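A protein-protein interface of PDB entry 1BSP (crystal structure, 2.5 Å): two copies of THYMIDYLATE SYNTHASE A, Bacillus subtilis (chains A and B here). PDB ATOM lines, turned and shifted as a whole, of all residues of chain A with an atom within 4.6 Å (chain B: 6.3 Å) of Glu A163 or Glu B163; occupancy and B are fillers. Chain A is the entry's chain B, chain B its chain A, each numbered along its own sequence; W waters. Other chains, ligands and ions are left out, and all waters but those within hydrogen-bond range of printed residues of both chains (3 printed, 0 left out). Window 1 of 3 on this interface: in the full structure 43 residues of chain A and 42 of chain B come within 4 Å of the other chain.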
ATOM      1  N   THR A 144      20.103 -12.738  26.515  1.00  0.00           N
ATOM      2  CA  THR A 144      20.474 -12.916  27.915  1.00  0.00           C
ATOM      3  C   THR A 144      21.997 -12.737  27.940  1.00  0.00           C
ATOM      4  O   THR A 144      22.694 -13.041  26.959  1.00  0.00           O
ATOM      5  CB  THR A 144      20.075 -14.302  28.480  1.00  0.00           C
ATOM      6  OG1 THR A 144      20.332 -15.317  27.501  1.00  0.00           O
ATOM      7  CG2 THR A 144      18.597 -14.335  28.850  1.00  0.00           C
ATOM      8  N   MET A 145      22.511 -12.204  29.037  1.00  0.00           N
ATOM      9  CA  MET A 145      23.931 -11.961  29.163  1.00  0.00           C
ATOM     10  C   MET A 145      24.465 -12.345  30.531  1.00  0.00           C
ATOM     11  O   MET A 145      24.002 -11.849  31.559  1.00  0.00           O
ATOM     12  CB  MET A 145      24.214 -10.475  28.890  1.00  0.00           C
ATOM     13  CG  MET A 145      25.692 -10.070  28.842  1.00  0.00           C
ATOM     14  SD  MET A 145      26.587 -10.931  27.557  1.00  0.00           S
ATOM     15  CE  MET A 145      25.474 -10.747  26.195  1.00  0.00           C
ATOM     16  N   VAL A 161      29.817 -20.354  27.927  1.00  0.00           N
ATOM     17  CA  VAL A 161      28.584 -20.085  27.186  1.00  0.00           C
ATOM     18  C   VAL A 161      28.023 -18.944  28.004  1.00  0.00           C
ATOM     19  O   VAL A 161      27.518 -19.158  29.108  1.00  0.00           O
ATOM     20  CB  VAL A 161      27.596 -21.265  27.218  1.00  0.00           C
ATOM     21  CG1 VAL A 161      26.305 -20.859  26.564  1.00  0.00           C
ATOM     22  CG2 VAL A 161      28.167 -22.448  26.459  1.00  0.00           C
ATOM     23  N   TYR A 162      28.163 -17.726  27.498  1.00  0.00           N
ATOM     24  CA  TYR A 162      27.721 -16.562  28.256  1.00  0.00           C
ATOM     25  C   TYR A 162      26.515 -15.792  27.724  1.00  0.00           C
ATOM     26  O   TYR A 162      26.021 -14.898  28.413  1.00  0.00           O
ATOM     27  CB  TYR A 162      28.901 -15.603  28.461  1.00  0.00           C
ATOM     28  CG  TYR A 162      29.400 -14.993  27.165  1.00  0.00           C
ATOM     29  CD1 TYR A 162      30.171 -15.736  26.275  1.00  0.00           C
ATOM     30  CD2 TYR A 162      29.022 -13.705  26.792  1.00  0.00           C
ATOM     31  CE1 TYR A 162      30.539 -15.225  25.049  1.00  0.00           C
ATOM     32  CE2 TYR A 162      29.382 -13.188  25.566  1.00  0.00           C
ATOM     33  CZ  TYR A 162      30.137 -13.951  24.700  1.00  0.00           C
ATOM     34  OH  TYR A 162      30.465 -13.442  23.467  1.00  0.00           O
ATOM     35  N   GLU A 163      26.043 -16.130  26.524  1.00  0.00           N
ATOM     36  CA  GLU A 163      24.889 -15.438  25.937  1.00  0.00           C
ATOM     37  C   GLU A 163      23.990 -16.305  25.041  1.00  0.00           C
ATOM     38  O   GLU A 163      24.381 -17.403  24.624  1.00  0.00           O
ATOM     39  CB  GLU A 163      25.367 -14.238  25.116  1.00  0.00           C
ATOM     40  CG  GLU A 163      26.229 -14.613  23.913  1.00  0.00           C
ATOM     41  CD  GLU A 163      26.638 -13.409  23.087  1.00  0.00           C
ATOM     42  OE1 GLU A 163      26.325 -12.268  23.493  1.00  0.00           O
ATOM     43  OE2 GLU A 163      27.262 -13.601  22.022  1.00  0.00           O
ATOM     44  N   THR A 164      22.784 -15.803  24.763  1.00  0.00           N
ATOM     45  CA  THR A 164      21.822 -16.473  23.878  1.00  0.00           C
ATOM     46  C   THR A 164      21.000 -15.396  23.186  1.00  0.00           C
ATOM     47  O   THR A 164      20.838 -14.299  23.711  1.00  0.00           O
ATOM     48  CB  THR A 164      20.780 -17.350  24.632  1.00  0.00           C
ATOM     49  OG1 THR A 164      20.006 -16.518  25.495  1.00  0.00           O
ATOM     50  CG2 THR A 164      21.431 -18.458  25.442  1.00  0.00           C
ATOM     51  N   GLU A 176      20.112 -19.144  19.361  1.00  0.00           N
ATOM     52  CA  GLU A 176      21.510 -19.005  18.989  1.00  0.00           C
ATOM     53  C   GLU A 176      22.300 -18.641  20.246  1.00  0.00           C
ATOM     54  O   GLU A 176      22.031 -17.610  20.873  1.00  0.00           O
ATOM     55  CB  GLU A 176      21.676 -17.917  17.926  1.00  0.00           C
ATOM     56  CG  GLU A 176      23.120 -17.599  17.611  1.00  0.00           C
ATOM     57  CD  GLU A 176      23.282 -16.766  16.368  1.00  0.00           C
ATOM     58  OE1 GLU A 176      22.559 -15.766  16.215  1.00  0.00           O
ATOM     59  OE2 GLU A 176      24.137 -17.116  15.532  1.00  0.00           O
ATOM     60  N   VAL A 177      23.210 -19.517  20.661  1.00  0.00           N
ATOM     61  CA  VAL A 177      24.017 -19.238  21.847  1.00  0.00           C
ATOM     62  C   VAL A 177      25.475 -19.105  21.436  1.00  0.00           C
ATOM     63  O   VAL A 177      25.878 -19.557  20.353  1.00  0.00           O
ATOM     64  CB  VAL A 177      23.870 -20.335  22.946  1.00  0.00           C
ATOM     65  CG1 VAL A 177      22.416 -20.738  23.092  1.00  0.00           C
ATOM     66  CG2 VAL A 177      24.730 -21.543  22.648  1.00  0.00           C
ATOM     67  N   ARG A 178      26.267 -18.471  22.289  1.00  0.00           N
ATOM     68  CA  ARG A 178      27.678 -18.300  21.994  1.00  0.00           C
ATOM     69  C   ARG A 178      28.585 -18.638  23.160  1.00  0.00           C
ATOM     70  O   ARG A 178      28.308 -18.255  24.299  1.00  0.00           O
ATOM     71  CB  ARG A 178      27.979 -16.870  21.534  1.00  0.00           C
ATOM     72  CG  ARG A 178      29.425 -16.728  21.069  1.00  0.00           C
ATOM     73  CD  ARG A 178      29.822 -15.332  20.608  1.00  0.00           C
ATOM     74  NE  ARG A 178      31.148 -15.368  19.985  1.00  0.00           N
ATOM     75  CZ  ARG A 178      32.284 -15.006  20.581  1.00  0.00           C
ATOM     76  NH1 ARG A 178      32.287 -14.550  21.823  1.00  0.00           N
ATOM     77  NH2 ARG A 178      33.438 -15.212  19.976  1.00  0.00           N
ATOM     78  N   ILE B 143      37.394  -9.720  25.899  1.00  0.00           N
ATOM     79  CA  ILE B 143      36.031  -9.346  25.532  1.00  0.00           C
ATOM     80  C   ILE B 143      35.575  -7.976  26.011  1.00  0.00           C
ATOM     81  O   ILE B 143      35.751  -7.643  27.191  1.00  0.00           O
ATOM     82  CB  ILE B 143      35.027 -10.377  26.141  1.00  0.00           C
ATOM     83  CG1 ILE B 143      35.301 -11.781  25.604  1.00  0.00           C
ATOM     84  CG2 ILE B 143      33.582  -9.949  25.891  1.00  0.00           C
ATOM     85  CD1 ILE B 143      34.592 -12.860  26.359  1.00  0.00           C
ATOM     86  N   THR B 144      34.966  -7.203  25.109  1.00  0.00           N
ATOM     87  CA  THR B 144      34.394  -5.891  25.454  1.00  0.00           C
ATOM     88  C   THR B 144      32.880  -6.086  25.334  1.00  0.00           C
ATOM     89  O   THR B 144      32.390  -6.710  24.375  1.00  0.00           O
ATOM     90  CB  THR B 144      34.893  -4.732  24.544  1.00  0.00           C
ATOM     91  OG1 THR B 144      34.852  -5.121  23.162  1.00  0.00           O
ATOM     92  CG2 THR B 144      36.312  -4.342  24.917  1.00  0.00           C
ATOM     93  N   MET B 145      32.145  -5.600  26.326  1.00  0.00           N
ATOM     94  CA  MET B 145      30.709  -5.775  26.366  1.00  0.00           C
ATOM     95  C   MET B 145      29.933  -4.490  26.572  1.00  0.00           C
ATOM     96  O   MET B 145      30.049  -3.843  27.620  1.00  0.00           O
ATOM     97  CB  MET B 145      30.378  -6.753  27.499  1.00  0.00           C
ATOM     98  CG  MET B 145      28.924  -7.137  27.651  1.00  0.00           C
ATOM     99  SD  MET B 145      28.294  -7.796  26.137  1.00  0.00           S
ATOM    100  CE  MET B 145      29.339  -9.195  25.855  1.00  0.00           C
ATOM    101  N   LEU B 146      29.135  -4.131  25.572  1.00  0.00           N
ATOM    102  CA  LEU B 146      28.289  -2.948  25.669  1.00  0.00           C
ATOM    103  C   LEU B 146      26.927  -3.317  26.266  1.00  0.00           C
ATOM    104  O   LEU B 146      26.317  -2.512  26.967  1.00  0.00           O
ATOM    105  CB  LEU B 146      28.117  -2.280  24.303  1.00  0.00           C
ATOM    106  CG  LEU B 146      29.336  -1.519  23.762  1.00  0.00           C
ATOM    107  CD1 LEU B 146      29.036  -0.993  22.377  1.00  0.00           C
ATOM    108  CD2 LEU B 146      29.707  -0.371  24.697  1.00  0.00           C
ATOM    109  N   TRP B 147      26.485  -4.554  26.040  1.00  0.00           N
ATOM    110  CA  TRP B 147      25.199  -5.029  26.556  1.00  0.00           C
ATOM    111  C   TRP B 147      25.223  -5.287  28.065  1.00  0.00           C
ATOM    112  O   TRP B 147      25.265  -6.427  28.507  1.00  0.00           O
ATOM    113  CB  TRP B 147      24.757  -6.301  25.807  1.00  0.00           C
ATOM    114  CG  TRP B 147      23.290  -6.667  25.999  1.00  0.00           C
ATOM    115  CD1 TRP B 147      22.752  -7.400  27.021  1.00  0.00           C
ATOM    116  CD2 TRP B 147      22.185  -6.271  25.168  1.00  0.00           C
ATOM    117  NE1 TRP B 147      21.387  -7.476  26.885  1.00  0.00           N
ATOM    118  CE2 TRP B 147      21.009  -6.792  25.760  1.00  0.00           C
ATOM    119  CE3 TRP B 147      22.070  -5.523  23.986  1.00  0.00           C
ATOM    120  CZ2 TRP B 147      19.737  -6.587  25.209  1.00  0.00           C
ATOM    121  CZ3 TRP B 147      20.798  -5.321  23.438  1.00  0.00           C
ATOM    122  CH2 TRP B 147      19.653  -5.851  24.052  1.00  0.00           C
ATOM    123  N   CYS B 160      23.626  -2.225  18.449  1.00  0.00           N
ATOM    124  CA  CYS B 160      23.504  -3.290  17.464  1.00  0.00           C
ATOM    125  C   CYS B 160      24.793  -4.102  17.621  1.00  0.00           C
ATOM    126  O   CYS B 160      24.745  -5.284  17.959  1.00  0.00           O
ATOM    127  CB  CYS B 160      23.378  -2.720  16.045  1.00  0.00           C
ATOM    128  SG  CYS B 160      21.767  -1.926  15.675  1.00  0.00           S
ATOM    129  N   VAL B 161      25.940  -3.458  17.394  1.00  0.00           N
ATOM    130  CA  VAL B 161      27.246  -4.106  17.569  1.00  0.00           C
ATOM    131  C   VAL B 161      27.533  -3.858  19.041  1.00  0.00           C
ATOM    132  O   VAL B 161      27.900  -2.754  19.426  1.00  0.00           O
ATOM    133  CB  VAL B 161      28.366  -3.457  16.727  1.00  0.00           C
ATOM    134  CG1 VAL B 161      29.662  -4.233  16.913  1.00  0.00           C
ATOM    135  CG2 VAL B 161      27.985  -3.443  15.249  1.00  0.00           C
ATOM    136  N   TYR B 162      27.327  -4.874  19.865  1.00  0.00           N
ATOM    137  CA  TYR B 162      27.503  -4.720  21.299  1.00  0.00           C
ATOM    138  C   TYR B 162      28.698  -5.456  21.904  1.00  0.00           C
ATOM    139  O   TYR B 162      28.922  -5.357  23.117  1.00  0.00           O
ATOM    140  CB  TYR B 162      26.220  -5.187  22.008  1.00  0.00           C
ATOM    141  CG  TYR B 162      25.907  -6.663  21.780  1.00  0.00           C
ATOM    142  CD1 TYR B 162      25.367  -7.100  20.569  1.00  0.00           C
ATOM    143  CD2 TYR B 162      26.221  -7.624  22.748  1.00  0.00           C
ATOM    144  CE1 TYR B 162      25.160  -8.449  20.320  1.00  0.00           C
ATOM    145  CE2 TYR B 162      26.016  -8.982  22.509  1.00  0.00           C
ATOM    146  CZ  TYR B 162      25.488  -9.383  21.291  1.00  0.00           C
ATOM    147  OH  TYR B 162      25.310 -10.722  21.030  1.00  0.00           O
ATOM    148  N   GLU B 163      29.450  -6.199  21.094  1.00  0.00           N
ATOM    149  CA  GLU B 163      30.573  -6.952  21.643  1.00  0.00           C
ATOM    150  C   GLU B 163      31.671  -7.304  20.650  1.00  0.00           C
ATOM    151  O   GLU B 163      31.436  -7.382  19.442  1.00  0.00           O
ATOM    152  CB  GLU B 163      30.063  -8.266  22.245  1.00  0.00           C
ATOM    153  CG  GLU B 163      29.621  -9.283  21.186  1.00  0.00           C
ATOM    154  CD  GLU B 163      29.156 -10.597  21.766  1.00  0.00           C
ATOM    155  OE1 GLU B 163      29.252 -10.798  23.001  1.00  0.00           O
ATOM    156  OE2 GLU B 163      28.694 -11.435  20.971  1.00  0.00           O
ATOM    157  N   THR B 164      32.856  -7.579  21.182  1.00  0.00           N
ATOM    158  CA  THR B 164      34.003  -7.975  20.374  1.00  0.00           C
ATOM    159  C   THR B 164      34.843  -8.944  21.201  1.00  0.00           C
ATOM    160  O   THR B 164      34.783  -8.933  22.442  1.00  0.00           O
ATOM    161  CB  THR B 164      34.925  -6.755  19.982  1.00  0.00           C
ATOM    162  OG1 THR B 164      35.610  -6.261  21.136  1.00  0.00           O
ATOM    163  CG2 THR B 164      34.123  -5.610  19.374  1.00  0.00           C
ATOM    164  N   GLN B 165      35.542  -9.842  20.511  1.00  0.00           N
ATOM    165  CA  GLN B 165      36.457 -10.766  21.163  1.00  0.00           C
ATOM    166  C   GLN B 165      37.733 -10.748  20.330  1.00  0.00           C
ATOM    167  O   GLN B 165      37.690 -10.857  19.098  1.00  0.00           O
ATOM    168  CB  GLN B 165      35.907 -12.187  21.281  1.00  0.00           C
ATOM    169  CG  GLN B 165      36.868 -13.104  22.055  1.00  0.00           C
ATOM    170  CD  GLN B 165      36.238 -14.397  22.523  1.00  0.00           C
ATOM    171  OE1 GLN B 165      35.423 -15.006  21.823  1.00  0.00           O
ATOM    172  NE2 GLN B 165      36.614 -14.827  23.719  1.00  0.00           N
ATOM    173  N   GLU B 176      36.770 -10.502  16.339  1.00  0.00           N
ATOM    174  CA  GLU B 176      35.443 -11.032  16.070  1.00  0.00           C
ATOM    175  C   GLU B 176      34.453 -10.114  16.777  1.00  0.00           C
ATOM    176  O   GLU B 176      34.582  -9.848  17.984  1.00  0.00           O
ATOM    177  CB  GLU B 176      35.309 -12.453  16.600  1.00  0.00           C
ATOM    178  CG  GLU B 176      34.004 -13.108  16.211  1.00  0.00           C
ATOM    179  CD  GLU B 176      33.969 -14.582  16.542  1.00  0.00           C
ATOM    180  OE1 GLU B 176      34.464 -14.953  17.618  1.00  0.00           O
ATOM    181  OE2 GLU B 176      33.456 -15.370  15.719  1.00  0.00           O
ATOM    182  N   VAL B 177      33.527  -9.554  16.003  1.00  0.00           N
ATOM    183  CA  VAL B 177      32.502  -8.663  16.544  1.00  0.00           C
ATOM    184  C   VAL B 177      31.131  -9.235  16.199  1.00  0.00           C
ATOM    185  O   VAL B 177      30.971  -9.993  15.230  1.00  0.00           O
ATOM    186  CB  VAL B 177      32.601  -7.237  15.945  1.00  0.00           C
ATOM    187  CG1 VAL B 177      33.981  -6.655  16.160  1.00  0.00           C
ATOM    188  CG2 VAL B 177      32.292  -7.277  14.482  1.00  0.00           C
ATOM    189  N   ARG B 178      30.139  -8.883  16.996  1.00  0.00           N
ATOM    190  CA  ARG B 178      28.806  -9.361  16.732  1.00  0.00           C
ATOM    191  C   ARG B 178      27.754  -8.277  16.815  1.00  0.00           C
ATOM    192  O   ARG B 178      27.765  -7.448  17.737  1.00  0.00           O
ATOM    193  CB  ARG B 178      28.432 -10.500  17.673  1.00  0.00           C
ATOM    194  CG  ARG B 178      27.097 -11.113  17.289  1.00  0.00           C
ATOM    195  CD  ARG B 178      26.692 -12.304  18.113  1.00  0.00           C
ATOM    196  NE  ARG B 178      25.555 -12.948  17.464  1.00  0.00           N
ATOM    197  CZ  ARG B 178      24.289 -12.798  17.832  1.00  0.00           C
ATOM    198  NH1 ARG B 178      23.971 -12.028  18.869  1.00  0.00           N
ATOM    199  NH2 ARG B 178      23.335 -13.384  17.126  1.00  0.00           N
ATOM    200  N   ALA B 179      26.868  -8.288  15.824  1.00  0.00           N
ATOM    201  CA  ALA B 179      25.745  -7.366  15.738  1.00  0.00           C
ATOM    202  C   ALA B 179      24.491  -8.209  15.950  1.00  0.00           C
ATOM    203  O   ALA B 179      24.277  -9.196  15.243  1.00  0.00           O
ATOM    204  CB  ALA B 179      25.703  -6.713  14.367  1.00  0.00           C
ATOM    205  N   TYR B 195      34.647  -1.374  12.262  1.00  0.00           N
ATOM    206  CA  TYR B 195      35.367  -2.187  13.232  1.00  0.00           C
ATOM    207  C   TYR B 195      36.702  -2.719  12.744  1.00  0.00           C
ATOM    208  O   TYR B 195      37.564  -3.093  13.538  1.00  0.00           O
ATOM    209  CB  TYR B 195      34.479  -3.270  13.831  1.00  0.00           C
ATOM    210  CG  TYR B 195      33.739  -2.733  15.027  1.00  0.00           C
ATOM    211  CD1 TYR B 195      32.659  -1.868  14.869  1.00  0.00           C
ATOM    212  CD2 TYR B 195      34.160  -3.032  16.317  1.00  0.00           C
ATOM    213  CE1 TYR B 195      32.023  -1.307  15.973  1.00  0.00           C
ATOM    214  CE2 TYR B 195      33.533  -2.480  17.426  1.00  0.00           C
ATOM    215  CZ  TYR B 195      32.465  -1.616  17.247  1.00  0.00           C
ATOM    216  OH  TYR B 195      31.858  -1.042  18.343  1.00  0.00           O
HETATM  217  O   HOH W   1      23.525 -13.816  21.755  1.00  0.00           O
HETATM  218  O   HOH W   2      31.788 -16.951  17.558  1.00  0.00           O
HETATM  219  O   HOH W   3      25.660 -14.520  15.045  1.00  0.00           O
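The guanidinium group (NH2) of Arg B178 lies within salt-bridge range of the side-chain carboxylate (OE1) of Glu A176, at 2.7 Å. OH of Tyr B162 sits at hydrogen-bond distance from OE1 of Glu A163. The side-chain carboxylate (OE1) of Glu B176 is in salt-bridge range of the guanidinium group (NH2) of Arg A178 (2.6 Å). The side-chain carboxylate (OE1) of Glu B163 sits at hydrogen-bond distance from the side-chain hydroxyl (OH) of Tyr A162 (2.9 Å). The guanidinium group of Arg A178 is in hydrogen-bond range of the side-chain amide oxygen of Gln B165 (2.7 Å). The side-chain carboxylate of Glu B163 lies close to the side-chain carboxylate of Glu A163, 2.8 Å away.
Water W3 bridges the guanidinium group (NE) of Arg B178 and the side-chain carboxylate (OE2) of Glu A176. Water W2 lies within hydrogen-bond range of the side-chain carboxylate of Glu B176 (2.9 Å) and the guanidinium group of Arg A178 (3.0 Å). Water W1 lies within hydrogen-bond range of O of Thr A164 (3.4 Å) and NH1 of Arg B178 (3.4 Å).
Of chain B, only Tyr B162 and Glu B163 come within 4 Å of Glu A163. Val A177 touches none of the printed residues of chain B. Ile B143 touches none of the printed residues of chain A. Of the printed residues of chain A, Met B145 touches Met A145. Printed residues of chain A within 4 Å of Tyr B162: Glu A163 (3.1 Å). Of chain A, only Tyr A162 (2.9 Å) and Glu A163 (2.8 Å) come within 4 Å of Glu B163. Of the printed residues of chain A, Gln B165 touches Arg A178. The nearest residue of chain A that does not touch Glu B163 is Arg A178 (4.1 Å). The nearest printed residue of chain A that does not touch Glu B176 is Tyr A162 (7.2 Å).
The backbone NH (N) of Trp B147 sits close to the side-chain sulfur (SD) of Met B145 (3.7 Å). N of Arg B178 sits at hydrogen-bond distance from O of Glu B163 (3.1 Å). The backbone carbonyl oxygen (O) of Tyr B162 is in hydrogen-bond range of the backbone NH (N) of Leu B146 (2.8 Å). OH of Tyr B162 lies within hydrogen-bond range of OE2 of Glu B163, 3.5 Å away. The backbone carbonyl oxygen (O) of Glu B176 is in hydrogen-bond range of the backbone NH (N) of Gln B165, at 2.7 Å. The guanidinium group (NH1) of Arg B178 is in hydrogen-bond range of the side-chain hydroxyl (OH) of Tyr B162, at 2.9 Å.
Met B145 touches its own counterpart, Met A145. Tyr A162 touches Glu B163, and with the chains exchanged Glu A163 touches Tyr B162. Glu B163 touches its own counterpart, Glu A163. Glu A176 touches Arg B178, and with the chains exchanged Arg A178 touches Glu B176. Of the 8 pairs that touch across the chains among the printed residues, 6 have their exchanged pair printed and touching as well.
Hydrophobic or aromatic side chains of chain A that line the printed part of chain B: Met A145 and Tyr A162. Along chain A the printed residues that touch a printed residue of chain B span positions 145 to 178. Among the printed residues, 8 pairs touch across the chains.
Among the printed residues, merely in contact across the chains: Met A145 with Met B145 (3.7 Å) and Met A145 with Trp B147 (3.7 Å).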
